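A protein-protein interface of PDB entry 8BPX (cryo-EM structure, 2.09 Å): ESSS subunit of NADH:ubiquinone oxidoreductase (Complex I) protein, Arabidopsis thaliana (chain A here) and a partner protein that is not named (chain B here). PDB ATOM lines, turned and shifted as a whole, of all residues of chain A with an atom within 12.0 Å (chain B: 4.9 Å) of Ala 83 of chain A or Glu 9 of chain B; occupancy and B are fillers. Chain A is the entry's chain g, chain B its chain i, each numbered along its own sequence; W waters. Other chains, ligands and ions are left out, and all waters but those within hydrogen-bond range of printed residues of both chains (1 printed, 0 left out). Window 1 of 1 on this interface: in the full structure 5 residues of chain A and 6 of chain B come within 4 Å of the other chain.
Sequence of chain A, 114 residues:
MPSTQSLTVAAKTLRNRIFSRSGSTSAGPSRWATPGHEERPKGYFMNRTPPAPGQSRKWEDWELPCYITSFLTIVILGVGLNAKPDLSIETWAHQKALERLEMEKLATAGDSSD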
ATOM      1  N   THR A  73       3.903 -28.736 -22.129  1.00  0.00           N
ATOM      2  CA  THR A  73       3.764 -30.001 -21.416  1.00  0.00           C
ATOM      3  C   THR A  73       3.762 -29.769 -19.914  1.00  0.00           C
ATOM      4  O   THR A  73       2.898 -30.281 -19.192  1.00  0.00           O
ATOM      5  CB  THR A  73       4.907 -30.944 -21.808  1.00  0.00           C
ATOM      6  OG1 THR A  73       4.787 -31.309 -23.187  1.00  0.00           O
ATOM      7  CG2 THR A  73       4.899 -32.198 -20.951  1.00  0.00           C
ATOM      8  N   ILE A  74       4.721 -28.976 -19.433  1.00  0.00           N
ATOM      9  CA  ILE A  74       4.793 -28.661 -18.010  1.00  0.00           C
ATOM     10  C   ILE A  74       3.514 -27.966 -17.560  1.00  0.00           C
ATOM     11  O   ILE A  74       2.914 -28.335 -16.547  1.00  0.00           O
ATOM     12  CB  ILE A  74       6.043 -27.808 -17.712  1.00  0.00           C
ATOM     13  CG1 ILE A  74       7.235 -28.685 -17.319  1.00  0.00           C
ATOM     14  CG2 ILE A  74       5.767 -26.779 -16.628  1.00  0.00           C
ATOM     15  CD1 ILE A  74       7.457 -29.896 -18.181  1.00  0.00           C
ATOM     16  N   VAL A  75       3.057 -26.978 -18.328  1.00  0.00           N
ATOM     17  CA  VAL A  75       1.878 -26.214 -17.929  1.00  0.00           C
ATOM     18  C   VAL A  75       0.638 -27.102 -17.933  1.00  0.00           C
ATOM     19  O   VAL A  75      -0.120 -27.136 -16.959  1.00  0.00           O
ATOM     20  CB  VAL A  75       1.703 -24.987 -18.841  1.00  0.00           C
ATOM     21  CG1 VAL A  75       0.264 -24.506 -18.815  1.00  0.00           C
ATOM     22  CG2 VAL A  75       2.659 -23.879 -18.425  1.00  0.00           C
ATOM     23  N   ILE A  76       0.436 -27.858 -19.016  1.00  0.00           N
ATOM     24  CA  ILE A  76      -0.744 -28.704 -19.143  1.00  0.00           C
ATOM     25  C   ILE A  76      -0.781 -29.735 -18.023  1.00  0.00           C
ATOM     26  O   ILE A  76      -1.789 -29.875 -17.329  1.00  0.00           O
ATOM     27  CB  ILE A  76      -0.778 -29.364 -20.535  1.00  0.00           C
ATOM     28  CG1 ILE A  76      -1.344 -28.389 -21.568  1.00  0.00           C
ATOM     29  CG2 ILE A  76      -1.604 -30.640 -20.526  1.00  0.00           C
ATOM     30  CD1 ILE A  76      -1.067 -28.793 -22.991  1.00  0.00           C
ATOM     31  N   LEU A  77       0.325 -30.447 -17.797  1.00  0.00           N
ATOM     32  CA  LEU A  77       0.293 -31.482 -16.769  1.00  0.00           C
ATOM     33  C   LEU A  77       0.182 -30.877 -15.373  1.00  0.00           C
ATOM     34  O   LEU A  77      -0.708 -31.251 -14.599  1.00  0.00           O
ATOM     35  CB  LEU A  77       1.520 -32.387 -16.890  1.00  0.00           C
ATOM     36  CG  LEU A  77       1.421 -33.347 -18.084  1.00  0.00           C
ATOM     37  CD1 LEU A  77       2.597 -34.312 -18.145  1.00  0.00           C
ATOM     38  CD2 LEU A  77       0.096 -34.093 -18.083  1.00  0.00           C
ATOM     39  N   GLY A  78       1.036 -29.900 -15.049  1.00  0.00           N
ATOM     40  CA  GLY A  78       1.054 -29.307 -13.727  1.00  0.00           C
ATOM     41  C   GLY A  78      -0.211 -28.567 -13.347  1.00  0.00           C
ATOM     42  O   GLY A  78      -0.529 -28.492 -12.158  1.00  0.00           O
ATOM     43  N   VAL A  79      -0.944 -28.029 -14.315  1.00  0.00           N
ATOM     44  CA  VAL A  79      -2.201 -27.366 -13.999  1.00  0.00           C
ATOM     45  C   VAL A  79      -3.374 -28.332 -14.094  1.00  0.00           C
ATOM     46  O   VAL A  79      -4.156 -28.455 -13.151  1.00  0.00           O
ATOM     47  CB  VAL A  79      -2.400 -26.133 -14.905  1.00  0.00           C
ATOM     48  CG1 VAL A  79      -3.774 -25.528 -14.684  1.00  0.00           C
ATOM     49  CG2 VAL A  79      -1.313 -25.105 -14.645  1.00  0.00           C
ATOM     50  N   GLY A  80      -3.521 -29.040 -15.219  1.00  0.00           N
ATOM     51  CA  GLY A  80      -4.671 -29.908 -15.395  1.00  0.00           C
ATOM     52  C   GLY A  80      -4.711 -31.073 -14.426  1.00  0.00           C
ATOM     53  O   GLY A  80      -5.785 -31.450 -13.953  1.00  0.00           O
ATOM     54  N   LEU A  81      -3.555 -31.673 -14.129  1.00  0.00           N
ATOM     55  CA  LEU A  81      -3.546 -32.787 -13.188  1.00  0.00           C
ATOM     56  C   LEU A  81      -3.954 -32.341 -11.791  1.00  0.00           C
ATOM     57  O   LEU A  81      -4.710 -33.047 -11.117  1.00  0.00           O
ATOM     58  CB  LEU A  81      -2.171 -33.455 -13.162  1.00  0.00           C
ATOM     59  CG  LEU A  81      -1.815 -34.322 -14.378  1.00  0.00           C
ATOM     60  CD1 LEU A  81      -0.451 -34.963 -14.206  1.00  0.00           C
ATOM     61  CD2 LEU A  81      -2.872 -35.374 -14.653  1.00  0.00           C
ATOM     62  N   ASN A  82      -3.487 -31.176 -11.346  1.00  0.00           N
ATOM     63  CA  ASN A  82      -3.912 -30.625 -10.068  1.00  0.00           C
ATOM     64  C   ASN A  82      -5.265 -29.936 -10.136  1.00  0.00           C
ATOM     65  O   ASN A  82      -5.825 -29.609  -9.088  1.00  0.00           O
ATOM     66  CB  ASN A  82      -2.877 -29.634  -9.530  1.00  0.00           C
ATOM     67  CG  ASN A  82      -1.559 -30.287  -9.214  1.00  0.00           C
ATOM     68  OD1 ASN A  82      -1.416 -30.981  -8.213  1.00  0.00           O
ATOM     69  ND2 ASN A  82      -0.577 -30.063 -10.071  1.00  0.00           N
ATOM     70  N   ALA A  83      -5.811 -29.714 -11.333  1.00  0.00           N
ATOM     71  CA  ALA A  83      -7.104 -29.067 -11.464  1.00  0.00           C
ATOM     72  C   ALA A  83      -8.245 -30.019 -11.778  1.00  0.00           C
ATOM     73  O   ALA A  83      -9.401 -29.675 -11.521  1.00  0.00           O
ATOM     74  CB  ALA A  83      -7.070 -27.979 -12.546  1.00  0.00           C
ATOM     75  N   LYS A  84      -7.893 -31.230 -12.197  1.00  0.00           N
ATOM     76  CA  LYS A  84      -8.931 -32.220 -12.566  1.00  0.00           C
ATOM     77  C   LYS A  84      -9.594 -32.688 -11.269  1.00  0.00           C
ATOM     78  O   LYS A  84      -8.893 -32.830 -10.249  1.00  0.00           O
ATOM     79  CB  LYS A  84      -8.361 -33.366 -13.409  1.00  0.00           C
ATOM     80  CG  LYS A  84      -7.519 -34.407 -12.686  1.00  0.00           C
ATOM     81  CD  LYS A  84      -6.813 -35.351 -13.633  1.00  0.00           C
ATOM     82  CE  LYS A  84      -7.755 -36.251 -14.409  1.00  0.00           C
ATOM     83  NZ  LYS A  84      -7.229 -37.634 -14.519  1.00  0.00           N
ATOM     84  N   PRO A  85     -10.905 -32.974 -11.301  1.00  0.00           N
ATOM     85  CA  PRO A  85     -11.572 -33.549 -10.135  1.00  0.00           C
ATOM     86  C   PRO A  85     -10.872 -34.862  -9.745  1.00  0.00           C
ATOM     87  O   PRO A  85     -10.389 -35.568 -10.615  1.00  0.00           O
ATOM     88  CB  PRO A  85     -12.987 -33.749 -10.678  1.00  0.00           C
ATOM     89  CG  PRO A  85     -12.820 -33.885 -12.163  1.00  0.00           C
ATOM     90  CD  PRO A  85     -11.765 -32.853 -12.474  1.00  0.00           C
ATOM     91  N   ASP A  86     -10.850 -35.177  -8.458  1.00  0.00           N
ATOM     92  CA  ASP A  86     -10.417 -36.487  -7.979  1.00  0.00           C
ATOM     93  C   ASP A  86     -11.596 -37.444  -8.093  1.00  0.00           C
ATOM     94  O   ASP A  86     -12.542 -37.385  -7.306  1.00  0.00           O
ATOM     95  CB  ASP A  86      -9.899 -36.390  -6.550  1.00  0.00           C
ATOM     96  CG  ASP A  86      -9.436 -37.723  -6.003  1.00  0.00           C
ATOM     97  OD1 ASP A  86      -9.387 -37.869  -4.768  1.00  0.00           O
ATOM     98  OD2 ASP A  86      -9.112 -38.625  -6.803  1.00  0.00           O
ATOM     99  N   LEU A  87     -11.498 -38.366  -9.043  1.00  0.00           N
ATOM    100  CA  LEU A  87     -12.602 -39.301  -9.344  1.00  0.00           C
ATOM    101  C   LEU A  87     -12.166 -40.732  -9.036  1.00  0.00           C
ATOM    102  O   LEU A  87     -12.931 -41.632  -9.283  1.00  0.00           O
ATOM    103  CB  LEU A  87     -13.022 -39.124 -10.804  1.00  0.00           C
ATOM    104  CG  LEU A  87     -13.552 -37.742 -11.173  1.00  0.00           C
ATOM    105  CD1 LEU A  87     -13.934 -37.693 -12.641  1.00  0.00           C
ATOM    106  CD2 LEU A  87     -14.734 -37.363 -10.295  1.00  0.00           C
ATOM    107  N   SER A  88     -11.007 -40.915  -8.421  1.00  0.00           N
ATOM    108  CA  SER A  88     -10.466 -42.246  -8.208  1.00  0.00           C
ATOM    109  C   SER A  88     -11.430 -43.098  -7.387  1.00  0.00           C
ATOM    110  O   SER A  88     -12.164 -42.599  -6.530  1.00  0.00           O
ATOM    111  CB  SER A  88      -9.106 -42.154  -7.515  1.00  0.00           C
ATOM    112  OG  SER A  88      -9.245 -41.744  -6.170  1.00  0.00           O
ATOM    113  N   MET B   5      -6.483 -21.538 -10.731  1.00  0.00           N
ATOM    114  CA  MET B   5      -6.963 -22.888 -10.523  1.00  0.00           C
ATOM    115  C   MET B   5      -8.484 -22.955 -10.630  1.00  0.00           C
ATOM    116  O   MET B   5      -8.925 -23.876 -11.279  1.00  0.00           O
ATOM    117  CB  MET B   5      -6.380 -23.471  -9.237  1.00  0.00           C
ATOM    118  CG  MET B   5      -5.796 -24.852  -9.441  1.00  0.00           C
ATOM    119  SD  MET B   5      -4.298 -24.865 -10.480  1.00  0.00           S
ATOM    120  CE  MET B   5      -4.064 -26.626 -10.645  1.00  0.00           C
ATOM    121  N   GLU B   6      -9.238 -21.994 -10.101  1.00  0.00           N
ATOM    122  CA  GLU B   6     -10.704 -22.148 -10.165  1.00  0.00           C
ATOM    123  C   GLU B   6     -11.103 -22.173 -11.648  1.00  0.00           C
ATOM    124  O   GLU B   6     -11.842 -23.078 -12.021  1.00  0.00           O
ATOM    125  CB  GLU B   6     -11.437 -21.134  -9.285  1.00  0.00           C
ATOM    126  CG  GLU B   6     -12.944 -21.240  -9.393  1.00  0.00           C
ATOM    127  CD  GLU B   6     -13.703 -19.965  -9.069  1.00  0.00           C
ATOM    128  OE1 GLU B   6     -13.067 -18.891  -9.042  1.00  0.00           O
ATOM    129  OE2 GLU B   6     -14.927 -20.049  -8.850  1.00  0.00           O
ATOM    130  N   PHE B   7     -10.523 -21.301 -12.448  1.00  0.00           N
ATOM    131  CA  PHE B   7     -10.785 -21.314 -13.904  1.00  0.00           C
ATOM    132  C   PHE B   7     -10.384 -22.696 -14.438  1.00  0.00           C
ATOM    133  O   PHE B   7     -11.117 -23.221 -15.216  1.00  0.00           O
ATOM    134  CB  PHE B   7     -10.096 -20.119 -14.584  1.00  0.00           C
ATOM    135  CG  PHE B   7      -9.985 -20.244 -16.074  1.00  0.00           C
ATOM    136  CD1 PHE B   7      -8.959 -20.975 -16.649  1.00  0.00           C
ATOM    137  CD2 PHE B   7     -10.935 -19.672 -16.895  1.00  0.00           C
ATOM    138  CE1 PHE B   7      -8.882 -21.116 -18.020  1.00  0.00           C
ATOM    139  CE2 PHE B   7     -10.852 -19.811 -18.265  1.00  0.00           C
ATOM    140  CZ  PHE B   7      -9.825 -20.527 -18.826  1.00  0.00           C
ATOM    141  N   ALA B   8      -9.212 -23.193 -14.032  1.00  0.00           N
ATOM    142  CA  ALA B   8      -8.766 -24.485 -14.539  1.00  0.00           C
ATOM    143  C   ALA B   8      -9.727 -25.606 -14.141  1.00  0.00           C
ATOM    144  O   ALA B   8     -10.008 -26.501 -14.947  1.00  0.00           O
ATOM    145  CB  ALA B   8      -7.350 -24.778 -14.052  1.00  0.00           C
ATOM    146  N   GLU B   9     -10.231 -25.574 -12.903  1.00  0.00           N
ATOM    147  CA  GLU B   9     -11.264 -26.522 -12.484  1.00  0.00           C
ATOM    148  C   GLU B   9     -12.437 -26.500 -13.447  1.00  0.00           C
ATOM    149  O   GLU B   9     -12.872 -27.542 -13.954  1.00  0.00           O
ATOM    150  CB  GLU B   9     -11.795 -26.204 -11.083  1.00  0.00           C
ATOM    151  CG  GLU B   9     -11.182 -26.854  -9.850  1.00  0.00           C
ATOM    152  CD  GLU B   9      -9.717 -26.600  -9.628  1.00  0.00           C
ATOM    153  OE1 GLU B   9      -9.367 -25.495  -9.176  1.00  0.00           O
ATOM    154  OE2 GLU B   9      -8.923 -27.530  -9.807  1.00  0.00           O
ATOM    155  N   ASN B  10     -12.963 -25.303 -13.700  1.00  0.00           N
ATOM    156  CA  ASN B  10     -14.141 -25.183 -14.547  1.00  0.00           C
ATOM    157  C   ASN B  10     -13.853 -25.643 -15.970  1.00  0.00           C
ATOM    158  O   ASN B  10     -14.677 -26.326 -16.585  1.00  0.00           O
ATOM    159  CB  ASN B  10     -14.655 -23.748 -14.523  1.00  0.00           C
ATOM    160  CG  ASN B  10     -15.311 -23.397 -13.213  1.00  0.00           C
ATOM    161  OD1 ASN B  10     -15.484 -24.254 -12.349  1.00  0.00           O
ATOM    162  ND2 ASN B  10     -15.682 -22.132 -13.051  1.00  0.00           N
ATOM    163  N   LEU B  11     -12.686 -25.286 -16.503  1.00  0.00           N
ATOM    164  CA  LEU B  11     -12.337 -25.686 -17.862  1.00  0.00           C
ATOM    165  C   LEU B  11     -12.230 -27.203 -17.984  1.00  0.00           C
ATOM    166  O   LEU B  11     -12.750 -27.801 -18.934  1.00  0.00           O
ATOM    167  CB  LEU B  11     -11.032 -25.006 -18.273  1.00  0.00           C
ATOM    168  CG  LEU B  11     -10.464 -25.307 -19.654  1.00  0.00           C
ATOM    169  CD1 LEU B  11     -11.545 -25.216 -20.721  1.00  0.00           C
ATOM    170  CD2 LEU B  11      -9.320 -24.371 -19.953  1.00  0.00           C
ATOM    171  N   VAL B  12     -11.588 -27.859 -17.012  1.00  0.00           N
ATOM    172  CA  VAL B  12     -11.389 -29.340 -17.112  1.00  0.00           C
ATOM    173  C   VAL B  12     -12.753 -30.053 -17.068  1.00  0.00           C
ATOM    174  O   VAL B  12     -12.958 -30.982 -17.863  1.00  0.00           O
ATOM    175  CB  VAL B  12     -10.413 -29.881 -16.047  1.00  0.00           C
ATOM    176  CG1 VAL B  12     -10.439 -31.398 -15.963  1.00  0.00           C
ATOM    177  CG2 VAL B  12      -8.997 -29.373 -16.247  1.00  0.00           C
ATOM    178  N   LEU B  13     -13.662 -29.603 -16.197  1.00  0.00           N
ATOM    179  CA  LEU B  13     -15.007 -30.225 -16.089  1.00  0.00           C
ATOM    180  C   LEU B  13     -15.784 -30.078 -17.408  1.00  0.00           C
ATOM    181  O   LEU B  13     -16.512 -31.011 -17.762  1.00  0.00           O
ATOM    182  CB  LEU B  13     -15.764 -29.609 -14.908  1.00  0.00           C
ATOM    183  CG  LEU B  13     -15.261 -29.971 -13.514  1.00  0.00           C
ATOM    184  CD1 LEU B  13     -15.880 -29.054 -12.474  1.00  0.00           C
ATOM    185  CD2 LEU B  13     -15.550 -31.425 -13.184  1.00  0.00           C
HETATM  186  O   HOH W   1     -12.216 -29.772 -12.464  1.00  0.00           O
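The backbone carbonyl oxygen (O) of Ala 83 of chain A sits close to the side-chain carboxylate (OE2) of Glu 9 of chain B.
O of Gly 78 of chain A is in hydrogen-bond range of ND2 of Asn 82 of chain A, 2.6 Å away. The backbone carbonyl oxygen (O) of Met 5 of chain B lies close to the side-chain carboxylate (OE1) of Glu 9 of chain B, 2.7 Å away.
O of Val 79 of chain A touches CE of Met 5 of chain B (3.1 Å). CB of Ala 8 of chain B touches CG1 of Val 79 of chain A, 3.7 Å away. CB of Asn 82 of chain A touches CE of Met 5 of chain B, 3.4 Å away. Glu 9 of chain B touches Asn 82 of chain A (OE2 to O, 3.8 Å). Met 5 of chain B touches Ala 83 of chain A. CB of Ala 83 of chain A touches CB of Ala 8 of chain B (3.5 Å). CA of Lys 84 of chain A touches CG1 of Val 12 of chain B (3.8 Å). Leu 13 of chain B touches Pro 85 of chain A (CD2 to CG, 3.8 Å).
Ile 74 of chain A touches none of the printed residues of chain B. Ile 76 of chain A touches none of the printed residues of chain B. Of the printed residues of chain B, Asn 82 of chain A touches Met 5 (3.4 Å) and Glu 9 (3.8 Å). Ala 83 of chain A touches just these residues of chain B: Met 5, Ala 8 and Glu 9. Of the printed residues of chain B, Lys 84 of chain A touches Val 12. Of the printed residues of chain B, Pro 85 of chain A touches Leu 13 (3.8 Å). Ala 8 of chain B touches just these residues of chain A: Val 79 (3.7 Å) and Ala 83 (3.5 Å). Of chain A, only Asn 82 and Ala 83 come within 4 Å of Glu 9 of chain B. Asn 10 of chain B touches none of the printed residues of chain A. Of the printed residues of chain A, Val 12 of chain B touches Lys 84 (3.8 Å).
Among the printed residues, 9 pairs touch across the chains. Among the printed residues, no Asp or Glu carboxylate lies within 4 Å of a Lys or Arg side-chain nitrogen of the other chain.
Water W1 lies within hydrogen-bond range of O of Glu 9 of chain B (2.8 Å) and O of Ala 83 of chain A (3.0 Å).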
